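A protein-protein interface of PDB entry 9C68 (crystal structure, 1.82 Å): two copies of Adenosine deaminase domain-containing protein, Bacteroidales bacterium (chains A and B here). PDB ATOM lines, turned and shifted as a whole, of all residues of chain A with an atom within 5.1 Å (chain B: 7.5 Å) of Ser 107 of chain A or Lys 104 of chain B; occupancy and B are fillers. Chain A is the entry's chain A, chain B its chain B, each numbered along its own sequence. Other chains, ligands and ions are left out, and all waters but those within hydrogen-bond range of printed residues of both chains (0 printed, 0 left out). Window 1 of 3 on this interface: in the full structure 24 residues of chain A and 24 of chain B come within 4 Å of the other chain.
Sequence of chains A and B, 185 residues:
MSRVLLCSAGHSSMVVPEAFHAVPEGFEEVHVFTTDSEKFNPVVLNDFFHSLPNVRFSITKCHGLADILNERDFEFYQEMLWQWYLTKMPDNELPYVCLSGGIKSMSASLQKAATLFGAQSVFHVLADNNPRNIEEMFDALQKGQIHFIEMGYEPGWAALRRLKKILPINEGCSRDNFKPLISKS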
ATOM      1  N   SER A   8       4.835  10.837  16.472  1.00  0.00           N
ATOM      2  CA  SER A   8       4.109  11.702  17.390  1.00  0.00           C
ATOM      3  C   SER A   8       3.518  10.870  18.525  1.00  0.00           C
ATOM      4  O   SER A   8       2.997   9.766  18.313  1.00  0.00           O
ATOM      5  CB  SER A   8       3.001  12.470  16.674  1.00  0.00           C
ATOM      6  OG  SER A   8       2.073  11.569  16.123  1.00  0.00           O
ATOM      7  N   LEU A  99       2.140   8.560  12.657  1.00  0.00           N
ATOM      8  CA  LEU A  99       1.334   9.675  13.157  1.00  0.00           C
ATOM      9  C   LEU A  99       0.280   9.237  14.177  1.00  0.00           C
ATOM     10  O   LEU A  99      -0.738   9.927  14.356  1.00  0.00           O
ATOM     11  CB  LEU A  99       0.698  10.403  11.968  1.00  0.00           C
ATOM     12  CG  LEU A  99       0.060   9.593  10.839  1.00  0.00           C
ATOM     13  CD1 LEU A  99      -1.124   8.712  11.253  1.00  0.00           C
ATOM     14  CD2 LEU A  99      -0.331  10.476   9.637  1.00  0.00           C
ATOM     15  N   SER A 100       0.519   8.115  14.887  1.00  0.00           N
ATOM     16  CA  SER A 100      -0.530   7.492  15.703  1.00  0.00           C
ATOM     17  C   SER A 100      -0.925   8.322  16.928  1.00  0.00           C
ATOM     18  O   SER A 100      -2.096   8.341  17.310  1.00  0.00           O
ATOM     19  CB  SER A 100      -0.080   6.101  16.161  1.00  0.00           C
ATOM     20  OG  SER A 100      -0.093   5.190  15.085  1.00  0.00           O
ATOM     21  N   GLY A 101       0.023   8.925  17.611  1.00  0.00           N
ATOM     22  CA  GLY A 101      -0.239   9.460  18.933  1.00  0.00           C
ATOM     23  C   GLY A 101      -0.715  10.904  18.890  1.00  0.00           C
ATOM     24  O   GLY A 101      -0.423  11.635  17.954  1.00  0.00           O
ATOM     25  N   GLY A 102      -1.493  11.287  19.901  1.00  0.00           N
ATOM     26  CA  GLY A 102      -1.913  12.665  20.106  1.00  0.00           C
ATOM     27  C   GLY A 102      -3.375  12.911  19.776  1.00  0.00           C
ATOM     28  O   GLY A 102      -4.137  12.015  19.406  1.00  0.00           O
ATOM     29  N   ILE A 103      -3.788  14.176  19.917  1.00  0.00           N
ATOM     30  CA  ILE A 103      -5.125  14.559  19.479  1.00  0.00           C
ATOM     31  C   ILE A 103      -5.105  14.571  17.959  1.00  0.00           C
ATOM     32  O   ILE A 103      -4.031  14.497  17.357  1.00  0.00           O
ATOM     33  CB  ILE A 103      -5.564  15.933  20.036  1.00  0.00           C
ATOM     34  CG1 ILE A 103      -4.719  17.067  19.451  1.00  0.00           C
ATOM     35  CG2 ILE A 103      -5.525  15.958  21.543  1.00  0.00           C
ATOM     36  CD1 ILE A 103      -5.392  18.423  19.718  1.00  0.00           C
ATOM     37  N   LYS A 104      -6.279  14.667  17.322  1.00  0.00           N
ATOM     38  CA  LYS A 104      -6.314  14.584  15.863  1.00  0.00           C
ATOM     39  C   LYS A 104      -5.446  15.664  15.230  1.00  0.00           C
ATOM     40  O   LYS A 104      -4.743  15.398  14.246  1.00  0.00           O
ATOM     41  CB  LYS A 104      -7.750  14.688  15.331  1.00  0.00           C
ATOM     42  CG  LYS A 104      -8.745  13.656  15.846  1.00  0.00           C
ATOM     43  CD  LYS A 104      -8.603  12.321  15.144  1.00  0.00           C
ATOM     44  CE  LYS A 104      -9.368  11.226  15.867  1.00  0.00           C
ATOM     45  NZ  LYS A 104     -10.844  11.406  15.834  1.00  0.00           N
ATOM     46  N   SER A 105      -5.484  16.892  15.777  1.00  0.00           N
ATOM     47  CA  SER A 105      -4.696  17.982  15.203  1.00  0.00           C
ATOM     48  C   SER A 105      -3.203  17.650  15.177  1.00  0.00           C
ATOM     49  O   SER A 105      -2.494  18.039  14.242  1.00  0.00           O
ATOM     50  CB  SER A 105      -4.938  19.283  15.982  1.00  0.00           C
ATOM     51  OG  SER A 105      -6.273  19.702  15.840  1.00  0.00           O
ATOM     52  N   MET A 106      -2.689  16.948  16.190  1.00  0.00           N
ATOM     53  CA  MET A 106      -1.258  16.658  16.099  1.00  0.00           C
ATOM     54  C   MET A 106      -0.961  15.546  15.098  1.00  0.00           C
ATOM     55  O   MET A 106       0.064  15.601  14.429  1.00  0.00           O
ATOM     56  CB  MET A 106      -0.625  16.365  17.465  1.00  0.00           C
ATOM     57  CG  MET A 106      -1.470  15.727  18.475  1.00  0.00           C
ATOM     58  SD  MET A 106      -0.981  16.216  20.151  1.00  0.00           S
ATOM     59  CE  MET A 106       0.644  15.422  20.257  1.00  0.00           C
ATOM     60  N   SER A 107      -1.867  14.576  14.938  1.00  0.00           N
ATOM     61  CA  SER A 107      -1.702  13.576  13.880  1.00  0.00           C
ATOM     62  C   SER A 107      -1.796  14.230  12.500  1.00  0.00           C
ATOM     63  O   SER A 107      -0.931  14.023  11.634  1.00  0.00           O
ATOM     64  CB  SER A 107      -2.752  12.475  14.082  1.00  0.00           C
ATOM     65  OG  SER A 107      -2.846  11.653  12.949  1.00  0.00           O
ATOM     66  N   ALA A 108      -2.818  15.066  12.300  1.00  0.00           N
ATOM     67  CA  ALA A 108      -3.001  15.793  11.045  1.00  0.00           C
ATOM     68  C   ALA A 108      -1.794  16.666  10.702  1.00  0.00           C
ATOM     69  O   ALA A 108      -1.411  16.772   9.530  1.00  0.00           O
ATOM     70  CB  ALA A 108      -4.263  16.657  11.128  1.00  0.00           C
ATOM     71  N   SER A 109      -1.199  17.316  11.705  1.00  0.00           N
ATOM     72  CA  SER A 109      -0.054  18.187  11.465  1.00  0.00           C
ATOM     73  C   SER A 109       1.184  17.391  11.051  1.00  0.00           C
ATOM     74  O   SER A 109       1.980  17.849  10.222  1.00  0.00           O
ATOM     75  CB  SER A 109       0.237  19.014  12.719  1.00  0.00           C
ATOM     76  OG  SER A 109       1.275  19.954  12.508  1.00  0.00           O
ATOM     77  N   LEU A 110       1.398  16.211  11.649  1.00  0.00           N
ATOM     78  CA  LEU A 110       2.506  15.371  11.194  1.00  0.00           C
ATOM     79  C   LEU A 110       2.282  14.862   9.773  1.00  0.00           C
ATOM     80  O   LEU A 110       3.229  14.794   8.977  1.00  0.00           O
ATOM     81  CB  LEU A 110       2.723  14.195  12.159  1.00  0.00           C
ATOM     82  CG  LEU A 110       3.982  13.327  11.935  1.00  0.00           C
ATOM     83  CD1 LEU A 110       5.305  14.102  11.782  1.00  0.00           C
ATOM     84  CD2 LEU A 110       4.090  12.379  13.142  1.00  0.00           C
ATOM     85  N   GLN A 111       1.059  14.462   9.438  1.00  0.00           N
ATOM     86  CA  GLN A 111       0.764  14.140   8.047  1.00  0.00           C
ATOM     87  C   GLN A 111       1.172  15.288   7.128  1.00  0.00           C
ATOM     88  O   GLN A 111       1.828  15.079   6.095  1.00  0.00           O
ATOM     89  CB  GLN A 111      -0.719  13.821   7.875  1.00  0.00           C
ATOM     90  CG  GLN A 111      -1.161  13.723   6.441  1.00  0.00           C
ATOM     91  CD  GLN A 111      -0.716  12.424   5.799  1.00  0.00           C
ATOM     92  OE1 GLN A 111      -1.225  11.367   6.127  1.00  0.00           O
ATOM     93  NE2 GLN A 111       0.292  12.494   4.942  1.00  0.00           N
ATOM     94  N   HIS A 124       0.014   4.302  10.397  1.00  0.00           N
ATOM     95  CA  HIS A 124      -0.814   4.326  11.599  1.00  0.00           C
ATOM     96  C   HIS A 124      -0.922   2.893  12.120  1.00  0.00           C
ATOM     97  O   HIS A 124      -0.775   1.927  11.365  1.00  0.00           O
ATOM     98  CB  HIS A 124      -2.196   4.914  11.305  1.00  0.00           C
ATOM     99  CG  HIS A 124      -3.095   5.025  12.509  1.00  0.00           C
ATOM    100  ND1 HIS A 124      -2.617   5.290  13.772  1.00  0.00           N
ATOM    101  CD2 HIS A 124      -4.438   4.931  12.627  1.00  0.00           C
ATOM    102  CE1 HIS A 124      -3.631   5.334  14.627  1.00  0.00           C
ATOM    103  NE2 HIS A 124      -4.747   5.120  13.955  1.00  0.00           N
ATOM    104  N   MET A 151       0.034   4.385   4.759  1.00  0.00           N
ATOM    105  CA  MET A 151      -0.770   5.431   4.151  1.00  0.00           C
ATOM    106  C   MET A 151      -0.057   6.142   3.007  1.00  0.00           C
ATOM    107  O   MET A 151      -0.699   6.902   2.284  1.00  0.00           O
ATOM    108  CB  MET A 151      -1.221   6.451   5.217  1.00  0.00           C
ATOM    109  CG  MET A 151      -1.706   5.790   6.503  1.00  0.00           C
ATOM    110  SD  MET A 151      -2.016   6.857   7.899  1.00  0.00           S
ATOM    111  CE  MET A 151      -2.977   8.239   7.270  1.00  0.00           C
ATOM    112  N   ILE B  68     -10.671   0.372   8.651  1.00  0.00           N
ATOM    113  CA  ILE B  68      -9.374   0.378   7.988  1.00  0.00           C
ATOM    114  C   ILE B  68      -8.391  -0.369   8.876  1.00  0.00           C
ATOM    115  O   ILE B  68      -8.121   0.062  10.002  1.00  0.00           O
ATOM    116  CB  ILE B  68      -8.891   1.815   7.724  1.00  0.00           C
ATOM    117  CG1 ILE B  68      -9.948   2.613   6.963  1.00  0.00           C
ATOM    118  CG2 ILE B  68      -7.540   1.807   7.011  1.00  0.00           C
ATOM    119  CD1 ILE B  68      -9.948   4.099   7.333  1.00  0.00           C
ATOM    120  N   PHE B  74      -6.918   1.316   3.426  1.00  0.00           N
ATOM    121  CA  PHE B  74      -6.687   2.749   3.460  1.00  0.00           C
ATOM    122  C   PHE B  74      -6.704   3.365   2.063  1.00  0.00           C
ATOM    123  O   PHE B  74      -7.311   4.421   1.860  1.00  0.00           O
ATOM    124  CB  PHE B  74      -5.374   3.069   4.141  1.00  0.00           C
ATOM    125  CG  PHE B  74      -5.064   4.535   4.104  1.00  0.00           C
ATOM    126  CD1 PHE B  74      -5.648   5.389   5.040  1.00  0.00           C
ATOM    127  CD2 PHE B  74      -4.235   5.071   3.131  1.00  0.00           C
ATOM    128  CE1 PHE B  74      -5.385   6.766   5.016  1.00  0.00           C
ATOM    129  CE2 PHE B  74      -3.964   6.451   3.093  1.00  0.00           C
ATOM    130  CZ  PHE B  74      -4.552   7.300   4.034  1.00  0.00           C
ATOM    131  N   LEU B  99     -11.991  17.819  10.528  1.00  0.00           N
ATOM    132  CA  LEU B  99     -11.368  16.500  10.490  1.00  0.00           C
ATOM    133  C   LEU B  99     -11.472  15.763  11.825  1.00  0.00           C
ATOM    134  O   LEU B  99     -10.612  14.936  12.155  1.00  0.00           O
ATOM    135  CB  LEU B  99      -9.907  16.618  10.061  1.00  0.00           C
ATOM    136  CG  LEU B  99      -9.076  17.770  10.625  1.00  0.00           C
ATOM    137  CD1 LEU B  99      -8.815  17.607  12.110  1.00  0.00           C
ATOM    138  CD2 LEU B  99      -7.750  17.796   9.907  1.00  0.00           C
ATOM    139  N   GLY B 101     -13.752  13.533  13.177  1.00  0.00           N
ATOM    140  CA  GLY B 101     -14.294  12.203  13.350  1.00  0.00           C
ATOM    141  C   GLY B 101     -13.393  11.152  12.715  1.00  0.00           C
ATOM    142  O   GLY B 101     -12.795  11.376  11.663  1.00  0.00           O
ATOM    143  N   GLY B 102     -13.314   9.994  13.361  1.00  0.00           N
ATOM    144  CA  GLY B 102     -12.733   8.814  12.745  1.00  0.00           C
ATOM    145  C   GLY B 102     -11.445   8.380  13.421  1.00  0.00           C
ATOM    146  O   GLY B 102     -10.968   8.978  14.387  1.00  0.00           O
ATOM    147  N   ILE B 103     -10.876   7.297  12.885  1.00  0.00           N
ATOM    148  CA  ILE B 103      -9.530   6.916  13.292  1.00  0.00           C
ATOM    149  C   ILE B 103      -8.546   7.942  12.734  1.00  0.00           C
ATOM    150  O   ILE B 103      -8.878   8.711  11.826  1.00  0.00           O
ATOM    151  CB  ILE B 103      -9.156   5.490  12.832  1.00  0.00           C
ATOM    152  CG1 ILE B 103      -9.002   5.445  11.311  1.00  0.00           C
ATOM    153  CG2 ILE B 103     -10.194   4.489  13.309  1.00  0.00           C
ATOM    154  CD1 ILE B 103      -8.504   4.105  10.740  1.00  0.00           C
ATOM    155  N   LYS B 104      -7.321   7.933  13.262  1.00  0.00           N
ATOM    156  CA  LYS B 104      -6.312   8.917  12.884  1.00  0.00           C
ATOM    157  C   LYS B 104      -6.099   8.962  11.372  1.00  0.00           C
ATOM    158  O   LYS B 104      -5.898  10.045  10.806  1.00  0.00           O
ATOM    159  CB  LYS B 104      -4.998   8.611  13.593  1.00  0.00           C
ATOM    160  CG  LYS B 104      -4.997   8.706  15.136  1.00  0.00           C
ATOM    161  CD  LYS B 104      -5.630   9.984  15.642  1.00  0.00           C
ATOM    162  CE  LYS B 104      -4.886  10.479  16.897  1.00  0.00           C
ATOM    163  NZ  LYS B 104      -4.827   9.528  18.056  1.00  0.00           N
ATOM    164  N   SER B 105      -6.128   7.798  10.700  1.00  0.00           N
ATOM    165  CA  SER B 105      -5.885   7.771   9.256  1.00  0.00           C
ATOM    166  C   SER B 105      -6.954   8.551   8.510  1.00  0.00           C
ATOM    167  O   SER B 105      -6.658   9.175   7.484  1.00  0.00           O
ATOM    168  CB  SER B 105      -5.848   6.325   8.728  1.00  0.00           C
ATOM    169  OG  SER B 105      -4.875   5.549   9.405  1.00  0.00           O
ATOM    170  N   MET B 106      -8.187   8.542   9.027  1.00  0.00           N
ATOM    171  CA  MET B 106      -9.275   9.289   8.413  1.00  0.00           C
ATOM    172  C   MET B 106      -9.032  10.794   8.539  1.00  0.00           C
ATOM    173  O   MET B 106      -9.062  11.520   7.538  1.00  0.00           O
ATOM    174  CB  MET B 106     -10.596   8.854   9.036  1.00  0.00           C
ATOM    175  CG  MET B 106     -10.818   7.332   8.873  1.00  0.00           C
ATOM    176  SD  MET B 106     -12.308   6.650   9.642  1.00  0.00           S
ATOM    177  CE  MET B 106     -13.542   7.833   9.061  1.00  0.00           C
ATOM    178  N   SER B 107      -8.702  11.267   9.745  1.00  0.00           N
ATOM    179  CA  SER B 107      -8.367  12.679   9.914  1.00  0.00           C
ATOM    180  C   SER B 107      -7.171  13.092   9.056  1.00  0.00           C
ATOM    181  O   SER B 107      -7.200  14.147   8.410  1.00  0.00           O
ATOM    182  CB  SER B 107      -8.110  12.978  11.395  1.00  0.00           C
ATOM    183  OG  SER B 107      -9.305  12.690  12.076  1.00  0.00           O
ATOM    184  N   ALA B 108      -6.116  12.277   9.021  1.00  0.00           N
ATOM    185  CA  ALA B 108      -4.937  12.655   8.245  1.00  0.00           C
ATOM    186  C   ALA B 108      -5.236  12.671   6.750  1.00  0.00           C
ATOM    187  O   ALA B 108      -4.718  13.523   6.026  1.00  0.00           O
ATOM    188  CB  ALA B 108      -3.760  11.724   8.558  1.00  0.00           C
ATOM    189  N   SER B 109      -6.078  11.756   6.263  1.00  0.00           N
ATOM    190  CA  SER B 109      -6.375  11.772   4.832  1.00  0.00           C
ATOM    191  C   SER B 109      -7.211  12.991   4.447  1.00  0.00           C
ATOM    192  O   SER B 109      -7.046  13.529   3.343  1.00  0.00           O
ATOM    193  CB  SER B 109      -7.079  10.475   4.418  1.00  0.00           C
ATOM    194  OG  SER B 109      -7.326  10.418   3.014  1.00  0.00           O
ATOM    195  N   LEU B 110      -8.112  13.438   5.327  1.00  0.00           N
ATOM    196  CA  LEU B 110      -8.889  14.634   5.020  1.00  0.00           C
ATOM    197  C   LEU B 110      -8.025  15.886   5.124  1.00  0.00           C
ATOM    198  O   LEU B 110      -8.189  16.823   4.333  1.00  0.00           O
ATOM    199  CB  LEU B 110     -10.113  14.727   5.934  1.00  0.00           C
ATOM    200  CG  LEU B 110     -11.088  15.886   5.721  1.00  0.00           C
ATOM    201  CD1 LEU B 110     -11.613  15.987   4.271  1.00  0.00           C
ATOM    202  CD2 LEU B 110     -12.247  15.807   6.726  1.00  0.00           C
ATOM    203  N   GLN B 111      -7.063  15.901   6.051  1.00  0.00           N
ATOM    204  CA  GLN B 111      -6.092  16.993   6.096  1.00  0.00           C
ATOM    205  C   GLN B 111      -5.312  17.080   4.791  1.00  0.00           C
ATOM    206  O   GLN B 111      -5.124  18.163   4.223  1.00  0.00           O
ATOM    207  CB  GLN B 111      -5.117  16.785   7.259  1.00  0.00           C
ATOM    208  CG  GLN B 111      -3.900  17.711   7.255  1.00  0.00           C
ATOM    209  CD  GLN B 111      -4.265  19.166   7.592  1.00  0.00           C
ATOM    210  OE1 GLN B 111      -4.465  19.517   8.759  1.00  0.00           O
ATOM    211  NE2 GLN B 111      -4.369  20.014   6.558  1.00  0.00           N
ATOM    212  N   MET B 151      -6.632  25.333  12.306  1.00  0.00           N
ATOM    213  CA  MET B 151      -5.298  24.860  11.980  1.00  0.00           C
ATOM    214  C   MET B 151      -4.823  25.310  10.602  1.00  0.00           C
ATOM    215  O   MET B 151      -3.737  24.916  10.181  1.00  0.00           O
ATOM    216  CB  MET B 151      -5.212  23.330  12.185  1.00  0.00           C
ATOM    217  CG  MET B 151      -6.478  22.542  11.990  1.00  0.00           C
ATOM    218  SD  MET B 151      -6.615  20.911  12.855  1.00  0.00           S
ATOM    219  CE  MET B 151      -5.161  20.096  12.183  1.00  0.00           C
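The backbone carbonyl oxygen (O) of Gly 102 of chain B is in hydrogen-bond range of the side-chain amino group (NZ) of Lys 104 of chain A (2.8 Å).
The backbone carbonyl oxygen (O) of Ser 100 of chain A is in hydrogen-bond range of the side-chain amino group (NZ) of Lys 104 of chain B, 3.1 Å away.
OG of Ser 105 of chain B is in hydrogen-bond range of SD of Met 151 of chain A.
The backbone carbonyl oxygen (O) of Gly 102 of chain A sits at hydrogen-bond distance from the side-chain amino group (NZ) of Lys 104 of chain B, at 2.9 Å.
OG of Ser 105 of chain A sits at hydrogen-bond distance from SD of Met 151 of chain B (3.2 Å).
O of Leu 99 of chain A lies within hydrogen-bond range of OG of Ser 107 of chain A, at 3.1 Å.
OG of Ser 100 of chain A lies within hydrogen-bond range of ND1 of His 124 of chain A (2.8 Å).
O of Leu 99 of chain B lies within hydrogen-bond range of OG of Ser 107 of chain B (2.6 Å).
Among the printed residues, pairs that only touch across the chains: Lys 104 of chain A with Ser 107 of chain B (3.2 Å), His 124 of chain A with Ser 105 of chain B (3.3 Å), Met 151 of chain A with Phe 74 of chain B (3.4 Å), Ala 108 of chain A with Gln 111 of chain B (3.5 Å), His 124 of chain A with Lys 104 of chain B (3.5 Å), Gln 111 of chain A with Ala 108 of chain B (3.5 Å), Ala 108 of chain A with Met 151 of chain B (3.7 Å), Ser 107 of chain A with Lys 104 of chain B (3.8 Å), Met 151 of chain A with Ala 108 of chain B (3.8 Å), Leu 99 of chain A with Ala 108 of chain B (3.8 Å), Lys 104 of chain A with Lys 104 of chain B (3.8 Å) and Ala 108 of chain A with Leu 99 of chain B (3.9 Å).
Of the printed residues of chain B, Ser 100 of chain A touches Lys 104.
Of the printed residues of chain B, Lys 104 of chain A touches Gly 102, Lys 104 and Ser 107.
Of chain B, only Lys 104 (3.8 Å) comes within 4 Å of Ser 107 of chain A.
Of the printed residues of chain B, Ala 108 of chain A touches Leu 99 (3.9 Å), Gln 111 (3.5 Å) and Met 151 (3.7 Å).
Of the printed residues of chain B, Gln 111 of chain A touches Ala 108.
Gly 101 of chain B touches none of the printed residues of chain A.
Of chain A, only Ser 100, Gly 102, Lys 104, Ser 107 and His 124 come within 4 Å of Lys 104 of chain B.
Of the printed residues of chain A, Ser 107 of chain B touches Lys 104 (3.2 Å).
The nearest residue of chain B that does not touch Ser 107 of chain A is Ala 108 of chain B (4.5 Å).
The nearest printed residue of chain A that does not touch Phe 74 of chain B is Gln 111 of chain A (5.7 Å).
Of the 16 printed residues of chain A, 10 touch a printed residue of chain B.
Printed residues of chain A that touch a printed residue of chain B: Leu 99, Ser 100, Gly 102, Lys 104, Ser 105, Ser 107, Ala 108, Gln 111, His 124 and Met 151.
Printed residues of chain B that touch a printed residue of chain A: Phe 74, Leu 99, Gly 102, Lys 104, Ser 105, Ser 107, Ala 108, Gln 111 and Met 151.
Along chain B the printed residues that touch a printed residue of chain A span positions 74 to 151.
Leu 99 of chain A touches Ala 108 of chain B, and with the chains exchanged Ala 108 of chain A touches Leu 99 of chain B.
Lys 104 of chain A touches its own counterpart, Lys 104 of chain B.
Lys 104 of chain A touches Ser 107 of chain B, and with the chains exchanged Ser 107 of chain A touches Lys 104 of chain B.
Ala 108 of chain A touches Met 151 of chain B, and with the chains exchanged Met 151 of chain A touches Ala 108 of chain B.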
